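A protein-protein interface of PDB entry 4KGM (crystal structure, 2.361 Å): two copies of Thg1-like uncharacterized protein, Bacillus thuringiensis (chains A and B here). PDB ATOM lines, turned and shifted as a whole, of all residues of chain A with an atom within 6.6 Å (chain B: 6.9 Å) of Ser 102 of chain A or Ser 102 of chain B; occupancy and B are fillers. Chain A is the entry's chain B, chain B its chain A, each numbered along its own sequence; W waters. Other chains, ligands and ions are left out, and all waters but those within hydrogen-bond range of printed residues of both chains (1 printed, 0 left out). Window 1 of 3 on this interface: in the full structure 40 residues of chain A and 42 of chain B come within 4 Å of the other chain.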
ATOM      1  N   LEU A  97     -11.277 -22.823  18.603  1.00  0.00           N
ATOM      2  CA  LEU A  97     -10.100 -23.250  17.845  1.00  0.00           C
ATOM      3  C   LEU A  97      -8.837 -23.372  18.696  1.00  0.00           C
ATOM      4  O   LEU A  97      -8.227 -24.439  18.764  1.00  0.00           O
ATOM      5  CB  LEU A  97      -9.842 -22.305  16.667  1.00  0.00           C
ATOM      6  CG  LEU A  97      -8.704 -22.697  15.715  1.00  0.00           C
ATOM      7  CD1 LEU A  97      -9.094 -23.900  14.861  1.00  0.00           C
ATOM      8  CD2 LEU A  97      -8.288 -21.522  14.842  1.00  0.00           C
ATOM      9  N   GLN A  98      -8.447 -22.278  19.341  1.00  0.00           N
ATOM     10  CA  GLN A  98      -7.212 -22.260  20.117  1.00  0.00           C
ATOM     11  C   GLN A  98      -7.256 -23.229  21.293  1.00  0.00           C
ATOM     12  O   GLN A  98      -6.220 -23.711  21.744  1.00  0.00           O
ATOM     13  CB  GLN A  98      -6.899 -20.848  20.614  1.00  0.00           C
ATOM     14  CG  GLN A  98      -6.588 -19.845  19.509  1.00  0.00           C
ATOM     15  CD  GLN A  98      -5.976 -18.566  20.050  1.00  0.00           C
ATOM     16  OE1 GLN A  98      -4.849 -18.567  20.543  1.00  0.00           O
ATOM     17  NE2 GLN A  98      -6.724 -17.469  19.973  1.00  0.00           N
ATOM     18  N   LYS A  99      -8.455 -23.512  21.788  1.00  0.00           N
ATOM     19  CA  LYS A  99      -8.605 -24.402  22.930  1.00  0.00           C
ATOM     20  C   LYS A  99      -8.489 -25.859  22.491  1.00  0.00           C
ATOM     21  O   LYS A  99      -7.830 -26.663  23.146  1.00  0.00           O
ATOM     22  CB  LYS A  99      -9.939 -24.149  23.636  1.00  0.00           C
ATOM     23  CG  LYS A  99      -9.909 -24.410  25.132  1.00  0.00           C
ATOM     24  CD  LYS A  99     -11.132 -23.815  25.814  1.00  0.00           C
ATOM     25  CE  LYS A  99     -11.136 -24.100  27.310  1.00  0.00           C
ATOM     26  NZ  LYS A  99      -9.975 -23.485  28.009  1.00  0.00           N
ATOM     27  N   ILE A 100      -9.122 -26.192  21.373  1.00  0.00           N
ATOM     28  CA  ILE A 100      -9.048 -27.544  20.837  1.00  0.00           C
ATOM     29  C   ILE A 100      -7.614 -27.906  20.439  1.00  0.00           C
ATOM     30  O   ILE A 100      -7.142 -29.010  20.716  1.00  0.00           O
ATOM     31  CB  ILE A 100     -10.003 -27.724  19.638  1.00  0.00           C
ATOM     32  CG1 ILE A 100     -11.459 -27.673  20.112  1.00  0.00           C
ATOM     33  CG2 ILE A 100      -9.742 -29.040  18.934  1.00  0.00           C
ATOM     34  CD1 ILE A 100     -12.472 -27.852  19.004  1.00  0.00           C
ATOM     35  N   ALA A 101      -6.916 -26.964  19.814  1.00  0.00           N
ATOM     36  CA  ALA A 101      -5.561 -27.212  19.335  1.00  0.00           C
ATOM     37  C   ALA A 101      -4.545 -27.293  20.472  1.00  0.00           C
ATOM     38  O   ALA A 101      -3.685 -28.173  20.485  1.00  0.00           O
ATOM     39  CB  ALA A 101      -5.148 -26.143  18.326  1.00  0.00           C
ATOM     40  N   SER A 102      -4.640 -26.372  21.425  1.00  0.00           N
ATOM     41  CA  SER A 102      -3.658 -26.312  22.500  1.00  0.00           C
ATOM     42  C   SER A 102      -3.811 -27.463  23.496  1.00  0.00           C
ATOM     43  O   SER A 102      -2.820 -28.063  23.909  1.00  0.00           O
ATOM     44  CB  SER A 102      -3.712 -24.960  23.217  1.00  0.00           C
ATOM     45  OG  SER A 102      -4.963 -24.761  23.853  1.00  0.00           O
ATOM     46  N   VAL A 103      -5.048 -27.774  23.871  1.00  0.00           N
ATOM     47  CA  VAL A 103      -5.302 -28.835  24.840  1.00  0.00           C
ATOM     48  C   VAL A 103      -4.965 -30.211  24.263  1.00  0.00           C
ATOM     49  O   VAL A 103      -4.419 -31.067  24.962  1.00  0.00           O
ATOM     50  CB  VAL A 103      -6.756 -28.795  25.374  1.00  0.00           C
ATOM     51  CG1 VAL A 103      -7.027 -29.965  26.310  1.00  0.00           C
ATOM     52  CG2 VAL A 103      -7.012 -27.481  26.092  1.00  0.00           C
ATOM     53  N   SER A 104      -5.279 -30.414  22.987  1.00  0.00           N
ATOM     54  CA  SER A 104      -4.892 -31.641  22.295  1.00  0.00           C
ATOM     55  C   SER A 104      -3.384 -31.834  22.346  1.00  0.00           C
ATOM     56  O   SER A 104      -2.897 -32.929  22.626  1.00  0.00           O
ATOM     57  CB  SER A 104      -5.351 -31.613  20.836  1.00  0.00           C
ATOM     58  OG  SER A 104      -6.759 -31.713  20.747  1.00  0.00           O
ATOM     59  N   ALA A 105      -2.647 -30.763  22.070  1.00  0.00           N
ATOM     60  CA  ALA A 105      -1.191 -30.809  22.118  1.00  0.00           C
ATOM     61  C   ALA A 105      -0.720 -30.992  23.555  1.00  0.00           C
ATOM     62  O   ALA A 105       0.314 -31.611  23.806  1.00  0.00           O
ATOM     63  CB  ALA A 105      -0.597 -29.544  21.520  1.00  0.00           C
ATOM     64  N   SER A 106      -1.486 -30.443  24.494  1.00  0.00           N
ATOM     65  CA  SER A 106      -1.184 -30.592  25.911  1.00  0.00           C
ATOM     66  C   SER A 106      -1.350 -32.045  26.341  1.00  0.00           C
ATOM     67  O   SER A 106      -0.427 -32.643  26.894  1.00  0.00           O
ATOM     68  CB  SER A 106      -2.095 -29.695  26.749  1.00  0.00           C
ATOM     69  OG  SER A 106      -1.723 -29.724  28.115  1.00  0.00           O
ATOM     70  N   MET A 107      -2.531 -32.599  26.079  1.00  0.00           N
ATOM     71  CA  MET A 107      -2.835 -33.987  26.410  1.00  0.00           C
ATOM     72  C   MET A 107      -1.808 -34.943  25.817  1.00  0.00           C
ATOM     73  O   MET A 107      -1.354 -35.871  26.485  1.00  0.00           O
ATOM     74  CB  MET A 107      -4.231 -34.364  25.913  1.00  0.00           C
ATOM     75  CG  MET A 107      -5.374 -33.716  26.680  1.00  0.00           C
ATOM     76  SD  MET A 107      -6.979 -34.137  25.971  1.00  0.00           S
ATOM     77  CE  MET A 107      -8.085 -33.390  27.167  1.00  0.00           C
ATOM     78  N   THR A 109       1.305 -34.201  24.875  1.00  0.00           N
ATOM     79  CA  THR A 109       2.580 -33.933  25.528  1.00  0.00           C
ATOM     80  C   THR A 109       2.687 -34.643  26.876  1.00  0.00           C
ATOM     81  O   THR A 109       3.705 -35.268  27.178  1.00  0.00           O
ATOM     82  CB  THR A 109       2.777 -32.420  25.745  1.00  0.00           C
ATOM     83  OG1 THR A 109       2.631 -31.733  24.496  1.00  0.00           O
ATOM     84  CG2 THR A 109       4.152 -32.132  26.323  1.00  0.00           C
ATOM     85  N   PHE A 128       4.905 -30.820  21.375  1.00  0.00           N
ATOM     86  CA  PHE A 128       4.044 -31.026  20.216  1.00  0.00           C
ATOM     87  C   PHE A 128       3.329 -29.739  19.822  1.00  0.00           C
ATOM     88  O   PHE A 128       3.125 -28.852  20.651  1.00  0.00           O
ATOM     89  CB  PHE A 128       2.995 -32.101  20.518  1.00  0.00           C
ATOM     90  CG  PHE A 128       3.560 -33.487  20.667  1.00  0.00           C
ATOM     91  CD1 PHE A 128       4.041 -33.929  21.891  1.00  0.00           C
ATOM     92  CD2 PHE A 128       3.589 -34.356  19.587  1.00  0.00           C
ATOM     93  CE1 PHE A 128       4.556 -35.207  22.029  1.00  0.00           C
ATOM     94  CE2 PHE A 128       4.104 -35.635  19.717  1.00  0.00           C
ATOM     95  CZ  PHE A 128       4.587 -36.061  20.940  1.00  0.00           C
ATOM     96  N   ASP A 129       2.946 -29.639  18.553  1.00  0.00           N
ATOM     97  CA  ASP A 129       2.081 -28.552  18.112  1.00  0.00           C
ATOM     98  C   ASP A 129       0.705 -29.125  17.804  1.00  0.00           C
ATOM     99  O   ASP A 129       0.550 -30.337  17.661  1.00  0.00           O
ATOM    100  CB  ASP A 129       2.650 -27.848  16.877  1.00  0.00           C
ATOM    101  CG  ASP A 129       2.219 -28.504  15.578  1.00  0.00           C
ATOM    102  OD1 ASP A 129       2.356 -29.738  15.454  1.00  0.00           O
ATOM    103  OD2 ASP A 129       1.734 -27.784  14.680  1.00  0.00           O
ATOM    104  N   GLY A 130      -0.290 -28.256  17.695  1.00  0.00           N
ATOM    105  CA  GLY A 130      -1.639 -28.699  17.405  1.00  0.00           C
ATOM    106  C   GLY A 130      -2.354 -27.746  16.476  1.00  0.00           C
ATOM    107  O   GLY A 130      -2.208 -26.531  16.589  1.00  0.00           O
ATOM    108  N   ARG A 131      -3.125 -28.300  15.546  1.00  0.00           N
ATOM    109  CA  ARG A 131      -3.893 -27.490  14.609  1.00  0.00           C
ATOM    110  C   ARG A 131      -5.236 -28.149  14.332  1.00  0.00           C
ATOM    111  O   ARG A 131      -5.326 -29.370  14.191  1.00  0.00           O
ATOM    112  CB  ARG A 131      -3.113 -27.272  13.308  1.00  0.00           C
ATOM    113  CG  ARG A 131      -2.911 -28.527  12.468  1.00  0.00           C
ATOM    114  CD  ARG A 131      -1.903 -28.294  11.355  1.00  0.00           C
ATOM    115  NE  ARG A 131      -0.552 -28.148  11.883  1.00  0.00           N
ATOM    116  CZ  ARG A 131       0.507 -27.818  11.152  1.00  0.00           C
ATOM    117  NH1 ARG A 131       0.374 -27.589   9.853  1.00  0.00           N
ATOM    118  NH2 ARG A 131       1.700 -27.708  11.724  1.00  0.00           N
ATOM    119  N   TRP B  92       8.124 -15.669  16.263  1.00  0.00           N
ATOM    120  CA  TRP B  92       8.028 -17.056  16.691  1.00  0.00           C
ATOM    121  C   TRP B  92       6.968 -17.770  15.863  1.00  0.00           C
ATOM    122  O   TRP B  92       5.800 -17.381  15.879  1.00  0.00           O
ATOM    123  CB  TRP B  92       7.663 -17.129  18.175  1.00  0.00           C
ATOM    124  CG  TRP B  92       7.871 -18.483  18.779  1.00  0.00           C
ATOM    125  CD1 TRP B  92       8.859 -19.374  18.473  1.00  0.00           C
ATOM    126  CD2 TRP B  92       7.066 -19.107  19.786  1.00  0.00           C
ATOM    127  NE1 TRP B  92       8.722 -20.511  19.231  1.00  0.00           N
ATOM    128  CE2 TRP B  92       7.629 -20.373  20.046  1.00  0.00           C
ATOM    129  CE3 TRP B  92       5.926 -18.717  20.497  1.00  0.00           C
ATOM    130  CZ2 TRP B  92       7.091 -21.251  20.983  1.00  0.00           C
ATOM    131  CZ3 TRP B  92       5.392 -19.591  21.426  1.00  0.00           C
ATOM    132  CH2 TRP B  92       5.975 -20.844  21.661  1.00  0.00           C
ATOM    133  N   PHE B  93       7.389 -18.801  15.131  1.00  0.00           N
ATOM    134  CA  PHE B  93       6.507 -19.555  14.238  1.00  0.00           C
ATOM    135  C   PHE B  93       5.819 -18.659  13.205  1.00  0.00           C
ATOM    136  O   PHE B  93       4.740 -18.990  12.708  1.00  0.00           O
ATOM    137  CB  PHE B  93       5.460 -20.344  15.035  1.00  0.00           C
ATOM    138  CG  PHE B  93       6.036 -21.457  15.866  1.00  0.00           C
ATOM    139  CD1 PHE B  93       7.021 -22.285  15.356  1.00  0.00           C
ATOM    140  CD2 PHE B  93       5.588 -21.675  17.160  1.00  0.00           C
ATOM    141  CE1 PHE B  93       7.548 -23.313  16.123  1.00  0.00           C
ATOM    142  CE2 PHE B  93       6.112 -22.697  17.932  1.00  0.00           C
ATOM    143  CZ  PHE B  93       7.094 -23.517  17.411  1.00  0.00           C
ATOM    144  N   LEU B  97      -1.043 -18.442  14.715  1.00  0.00           N
ATOM    145  CA  LEU B  97      -1.882 -18.469  15.913  1.00  0.00           C
ATOM    146  C   LEU B  97      -1.938 -19.838  16.596  1.00  0.00           C
ATOM    147  O   LEU B  97      -1.577 -19.964  17.764  1.00  0.00           O
ATOM    148  CB  LEU B  97      -3.299 -17.982  15.596  1.00  0.00           C
ATOM    149  CG  LEU B  97      -4.263 -17.877  16.784  1.00  0.00           C
ATOM    150  CD1 LEU B  97      -3.865 -16.741  17.725  1.00  0.00           C
ATOM    151  CD2 LEU B  97      -5.697 -17.705  16.314  1.00  0.00           C
ATOM    152  N   GLN B  98      -2.382 -20.858  15.865  1.00  0.00           N
ATOM    153  CA  GLN B  98      -2.567 -22.190  16.443  1.00  0.00           C
ATOM    154  C   GLN B  98      -1.263 -22.822  16.914  1.00  0.00           C
ATOM    155  O   GLN B  98      -1.261 -23.636  17.836  1.00  0.00           O
ATOM    156  CB  GLN B  98      -3.268 -23.125  15.459  1.00  0.00           C
ATOM    157  CG  GLN B  98      -4.723 -22.782  15.199  1.00  0.00           C
ATOM    158  CD  GLN B  98      -5.465 -23.910  14.511  1.00  0.00           C
ATOM    159  OE1 GLN B  98      -5.763 -24.934  15.125  1.00  0.00           O
ATOM    160  NE2 GLN B  98      -5.764 -23.729  13.229  1.00  0.00           N
ATOM    161  N   LYS B  99      -0.156 -22.451  16.283  1.00  0.00           N
ATOM    162  CA  LYS B  99       1.134 -23.018  16.645  1.00  0.00           C
ATOM    163  C   LYS B  99       1.691 -22.356  17.903  1.00  0.00           C
ATOM    164  O   LYS B  99       2.231 -23.029  18.777  1.00  0.00           O
ATOM    165  CB  LYS B  99       2.122 -22.909  15.480  1.00  0.00           C
ATOM    166  CG  LYS B  99       2.967 -24.155  15.282  1.00  0.00           C
ATOM    167  CD  LYS B  99       3.770 -24.088  13.999  1.00  0.00           C
ATOM    168  CE  LYS B  99       4.578 -25.360  13.791  1.00  0.00           C
ATOM    169  NZ  LYS B  99       5.375 -25.303  12.535  1.00  0.00           N
ATOM    170  N   ILE B 100       1.549 -21.038  17.996  1.00  0.00           N
ATOM    171  CA  ILE B 100       2.007 -20.305  19.170  1.00  0.00           C
ATOM    172  C   ILE B 100       1.268 -20.763  20.428  1.00  0.00           C
ATOM    173  O   ILE B 100       1.882 -20.991  21.466  1.00  0.00           O
ATOM    174  CB  ILE B 100       1.829 -18.783  18.994  1.00  0.00           C
ATOM    175  CG1 ILE B 100       2.818 -18.245  17.961  1.00  0.00           C
ATOM    176  CG2 ILE B 100       2.029 -18.061  20.314  1.00  0.00           C
ATOM    177  CD1 ILE B 100       2.676 -16.760  17.702  1.00  0.00           C
ATOM    178  N   ALA B 101      -0.049 -20.908  20.322  1.00  0.00           N
ATOM    179  CA  ALA B 101      -0.872 -21.307  21.462  1.00  0.00           C
ATOM    180  C   ALA B 101      -0.614 -22.748  21.904  1.00  0.00           C
ATOM    181  O   ALA B 101      -0.450 -23.018  23.091  1.00  0.00           O
ATOM    182  CB  ALA B 101      -2.351 -21.102  21.147  1.00  0.00           C
ATOM    183  N   SER B 102      -0.577 -23.666  20.945  1.00  0.00           N
ATOM    184  CA  SER B 102      -0.436 -25.085  21.257  1.00  0.00           C
ATOM    185  C   SER B 102       0.957 -25.439  21.778  1.00  0.00           C
ATOM    186  O   SER B 102       1.091 -26.141  22.780  1.00  0.00           O
ATOM    187  CB  SER B 102      -0.792 -25.947  20.040  1.00  0.00           C
ATOM    188  OG  SER B 102       0.100 -25.714  18.964  1.00  0.00           O
ATOM    189  N   VAL B 103       1.990 -24.953  21.097  1.00  0.00           N
ATOM    190  CA  VAL B 103       3.366 -25.233  21.499  1.00  0.00           C
ATOM    191  C   VAL B 103       3.671 -24.637  22.872  1.00  0.00           C
ATOM    192  O   VAL B 103       4.407 -25.228  23.666  1.00  0.00           O
ATOM    193  CB  VAL B 103       4.382 -24.747  20.437  1.00  0.00           C
ATOM    194  CG1 VAL B 103       5.811 -24.837  20.957  1.00  0.00           C
ATOM    195  CG2 VAL B 103       4.233 -25.558  19.162  1.00  0.00           C
ATOM    196  N   SER B 104       3.085 -23.477  23.156  1.00  0.00           N
ATOM    197  CA  SER B 104       3.214 -22.867  24.475  1.00  0.00           C
ATOM    198  C   SER B 104       2.600 -23.772  25.536  1.00  0.00           C
ATOM    199  O   SER B 104       3.193 -24.002  26.590  1.00  0.00           O
ATOM    200  CB  SER B 104       2.540 -21.495  24.514  1.00  0.00           C
ATOM    201  OG  SER B 104       3.214 -20.574  23.679  1.00  0.00           O
ATOM    202  N   ALA B 105       1.405 -24.281  25.247  1.00  0.00           N
ATOM    203  CA  ALA B 105       0.715 -25.174  26.169  1.00  0.00           C
ATOM    204  C   ALA B 105       1.478 -26.486  26.305  1.00  0.00           C
ATOM    205  O   ALA B 105       1.567 -27.054  27.393  1.00  0.00           O
ATOM    206  CB  ALA B 105      -0.710 -25.427  25.700  1.00  0.00           C
ATOM    207  N   SER B 106       2.034 -26.957  25.194  1.00  0.00           N
ATOM    208  CA  SER B 106       2.828 -28.181  25.192  1.00  0.00           C
ATOM    209  C   SER B 106       4.073 -28.027  26.057  1.00  0.00           C
ATOM    210  O   SER B 106       4.369 -28.885  26.889  1.00  0.00           O
ATOM    211  CB  SER B 106       3.227 -28.552  23.765  1.00  0.00           C
ATOM    212  OG  SER B 106       4.006 -29.735  23.737  1.00  0.00           O
ATOM    213  N   MET B 107       4.798 -26.931  25.854  1.00  0.00           N
ATOM    214  CA  MET B 107       6.004 -26.651  26.626  1.00  0.00           C
ATOM    215  C   MET B 107       5.690 -26.549  28.111  1.00  0.00           C
ATOM    216  O   MET B 107       6.409 -27.101  28.945  1.00  0.00           O
ATOM    217  CB  MET B 107       6.664 -25.355  26.151  1.00  0.00           C
ATOM    218  CG  MET B 107       7.440 -25.480  24.849  1.00  0.00           C
ATOM    219  SD  MET B 107       8.096 -23.891  24.298  1.00  0.00           S
ATOM    220  CE  MET B 107       9.028 -24.403  22.855  1.00  0.00           C
ATOM    221  N   ALA B 108       4.615 -25.836  28.432  1.00  0.00           N
ATOM    222  CA  ALA B 108       4.186 -25.682  29.815  1.00  0.00           C
ATOM    223  C   ALA B 108       3.847 -27.044  30.409  1.00  0.00           C
ATOM    224  O   ALA B 108       4.233 -27.351  31.533  1.00  0.00           O
ATOM    225  CB  ALA B 108       2.990 -24.745  29.902  1.00  0.00           C
ATOM    226  N   THR B 109       3.137 -27.858  29.635  1.00  0.00           N
ATOM    227  CA  THR B 109       2.753 -29.198  30.059  1.00  0.00           C
ATOM    228  C   THR B 109       3.966 -30.084  30.345  1.00  0.00           C
ATOM    229  O   THR B 109       4.004 -30.790  31.354  1.00  0.00           O
ATOM    230  CB  THR B 109       1.871 -29.878  28.996  1.00  0.00           C
ATOM    231  OG1 THR B 109       0.681 -29.107  28.797  1.00  0.00           O
ATOM    232  CG2 THR B 109       1.490 -31.283  29.429  1.00  0.00           C
ATOM    233  N   PHE B 128      -2.879 -28.180  30.171  1.00  0.00           N
ATOM    234  CA  PHE B 128      -3.050 -26.738  30.062  1.00  0.00           C
ATOM    235  C   PHE B 128      -3.693 -26.376  28.729  1.00  0.00           C
ATOM    236  O   PHE B 128      -3.595 -27.125  27.756  1.00  0.00           O
ATOM    237  CB  PHE B 128      -1.694 -26.034  30.157  1.00  0.00           C
ATOM    238  CG  PHE B 128      -0.990 -26.231  31.469  1.00  0.00           C
ATOM    239  CD1 PHE B 128      -0.224 -27.362  31.699  1.00  0.00           C
ATOM    240  CD2 PHE B 128      -1.075 -25.273  32.464  1.00  0.00           C
ATOM    241  CE1 PHE B 128       0.427 -27.541  32.904  1.00  0.00           C
ATOM    242  CE2 PHE B 128      -0.426 -25.446  33.669  1.00  0.00           C
ATOM    243  CZ  PHE B 128       0.325 -26.581  33.890  1.00  0.00           C
ATOM    244  N   ASP B 129      -4.350 -25.223  28.684  1.00  0.00           N
ATOM    245  CA  ASP B 129      -4.818 -24.678  27.420  1.00  0.00           C
ATOM    246  C   ASP B 129      -3.937 -23.487  27.072  1.00  0.00           C
ATOM    247  O   ASP B 129      -3.180 -23.005  27.914  1.00  0.00           O
ATOM    248  CB  ASP B 129      -6.283 -24.251  27.507  1.00  0.00           C
ATOM    249  CG  ASP B 129      -6.449 -22.827  27.996  1.00  0.00           C
ATOM    250  OD1 ASP B 129      -5.838 -22.463  29.023  1.00  0.00           O
ATOM    251  OD2 ASP B 129      -7.190 -22.065  27.343  1.00  0.00           O
ATOM    252  N   GLY B 130      -4.038 -23.014  25.836  1.00  0.00           N
ATOM    253  CA  GLY B 130      -3.250 -21.879  25.396  1.00  0.00           C
ATOM    254  C   GLY B 130      -4.025 -20.974  24.461  1.00  0.00           C
ATOM    255  O   GLY B 130      -4.811 -21.442  23.639  1.00  0.00           O
ATOM    256  N   ARG B 131      -3.806 -19.671  24.595  1.00  0.00           N
ATOM    257  CA  ARG B 131      -4.439 -18.697  23.716  1.00  0.00           C
ATOM    258  C   ARG B 131      -3.499 -17.528  23.458  1.00  0.00           C
ATOM    259  O   ARG B 131      -2.804 -17.064  24.363  1.00  0.00           O
ATOM    260  CB  ARG B 131      -5.765 -18.211  24.307  1.00  0.00           C
ATOM    261  CG  ARG B 131      -5.637 -17.493  25.642  1.00  0.00           C
ATOM    262  CD  ARG B 131      -6.993 -17.297  26.296  1.00  0.00           C
ATOM    263  NE  ARG B 131      -7.597 -18.571  26.670  1.00  0.00           N
ATOM    264  CZ  ARG B 131      -8.786 -18.692  27.253  1.00  0.00           C
ATOM    265  NH1 ARG B 131      -9.504 -17.613  27.529  1.00  0.00           N
ATOM    266  NH2 ARG B 131      -9.256 -19.895  27.559  1.00  0.00           N
HETATM  267  O   HOH W   1      -7.428 -21.769  24.642  1.00  0.00           O
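The side-chain hydroxyl of Thr 109 of chain A sits at hydrogen-bond distance from the side-chain hydroxyl of Ser 106 of chain B (2.5 Å). OG of Ser 106 of chain A lies within hydrogen-bond range of OG1 of Thr 109 of chain B (2.6 Å). The side-chain amino group (NZ) of Lys 99 of chain A is in salt-bridge range of the side-chain carboxylate (OD2) of Asp 129 of chain B (3.2 Å). The side-chain hydroxyl of Ser 106 of chain B is in hydrogen-bond range of the backbone NH of Phe 128 of chain A. The side-chain hydroxyl (OG) of Ser 102 of chain A lies within hydrogen-bond range of the backbone NH (N) of Gly 130 of chain B (2.8 Å). O of Gly 130 of chain A lies close to O of Gln 98 of chain B (3.3 Å). N of Phe 128 of chain B lies within hydrogen-bond range of OG of Ser 106 of chain A (2.8 Å). The backbone carbonyl oxygen (O) of Gln 98 of chain A lies close to the backbone carbonyl oxygen (O) of Gly 130 of chain B. OG of Ser 102 of chain B is in hydrogen-bond range of N of Gly 130 of chain A, 2.9 Å away.
The side-chain hydroxyl (OG1) of Thr 109 of chain A is in hydrogen-bond range of the backbone carbonyl oxygen (O) of Ala 105 of chain A. The side-chain carboxylate (OD2) of Asp 129 of chain B lies within salt-bridge range of the guanidinium group (NH2) of Arg 131 of chain B. O of Gln 98 of chain B is in hydrogen-bond range of OG of Ser 102 of chain B (2.7 Å). The backbone carbonyl oxygen of Ala 105 of chain B is in hydrogen-bond range of the side-chain hydroxyl of Thr 109 of chain B (2.6 Å). O of Lys 99 of chain B is in hydrogen-bond range of OG of Ser 102 of chain B. O of Gln 98 of chain A lies within hydrogen-bond range of OG of Ser 102 of chain A.
Leu 97 of chain A touches Gln 98 of chain B (CD1 to OE1, 3.5 Å). OE1 of Gln 98 of chain A touches CB of Ala 101 of chain B, at 3.6 Å. CB of Ala 101 of chain A touches OE1 of Gln 98 of chain B (3.5 Å). CB of Ser 102 of chain A touches O of Ala 101 of chain B, at 3.8 Å. CG2 of Val 103 of chain A touches CB of Asp 129 of chain B, at 3.6 Å. CB of Ala 105 of chain A touches CB of Ser 102 of chain B, 3.9 Å away. Lys 99 of chain B touches Asp 129 of chain A. CA of Asp 129 of chain A touches OG of Ser 102 of chain B (3.6 Å). Asp 129 of chain A touches Val 103 of chain B (CB to CG2, 3.6 Å). Arg 131 of chain A touches Gln 98 of chain B (CA to OE1, 3.2 Å).
Of the printed residues of chain B, Leu 97 of chain A touches Gln 98 (3.5 Å). Of chain B, only Ala 101 (3.8 Å), Ser 102 (3.7 Å), Ala 105 (3.8 Å), Asp 129 (3.6 Å) and Gly 130 (2.8 Å) come within 4 Å of Ser 102 of chain A. Of the printed residues of chain A, Ser 102 of chain B touches Ala 101, Ser 102, Ala 105, Asp 129 and Gly 130. Ala 108 of chain B touches none of the printed residues of chain A. Of the printed residues of chain A, Phe 128 of chain B touches Val 103 (3.8 Å) and Ser 106 (2.8 Å).
Of the 19 printed residues of chain B, 13 touch a printed residue of chain A. Printed residues of chain B that touch a printed residue of chain A: Leu 97, Gln 98, Lys 99, Ala 101, Ser 102, Val 103, Ala 105, Ser 106, Thr 109, Phe 128, Asp 129, Gly 130 and Arg 131. Hydrophobic or aromatic side chains of chain A that line the printed part of chain B: Leu 97, Ala 101, Val 103 and Ala 105. Along chain A the printed residues that touch a printed residue of chain B span positions 97 to 131. Among the printed residues, Asp or Glu carboxylates within 4 Å of a Lys or Arg side-chain nitrogen of the other chain: Lys 99 of chain A with Asp 129 of chain B (3.2 Å).
Ala 101 of chain A touches Ser 102 of chain B, and with the chains exchanged Ser 102 of chain A touches Ala 101 of chain B. Ser 102 of chain A touches Ala 105 of chain B, and with the chains exchanged Ala 105 of chain A touches Ser 102 of chain B. Ser 102 of chain A touches Asp 129 of chain B, and with the chains exchanged Asp 129 of chain A touches Ser 102 of chain B. Ser 106 of chain A touches Phe 128 of chain B, and with the chains exchanged Phe 128 of chain A touches Ser 106 of chain B. Positions printed for both chains: 97, 98, 99, 100, 101, 102, 103, 104, 105, 106, 107, 109, 128, 129, 130 and 131. Of the 28 pairs that touch across the chains among the printed residues, 27 have their exchanged pair printed and touching as well.
Water W1 lies within hydrogen-bond range of the side-chain carboxylate of Asp 129 of chain B (2.7 Å), the backbone carbonyl oxygen of Gly 130 of chain B (2.8 Å) and the backbone NH of Lys 99 of chain A (3.5 Å).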
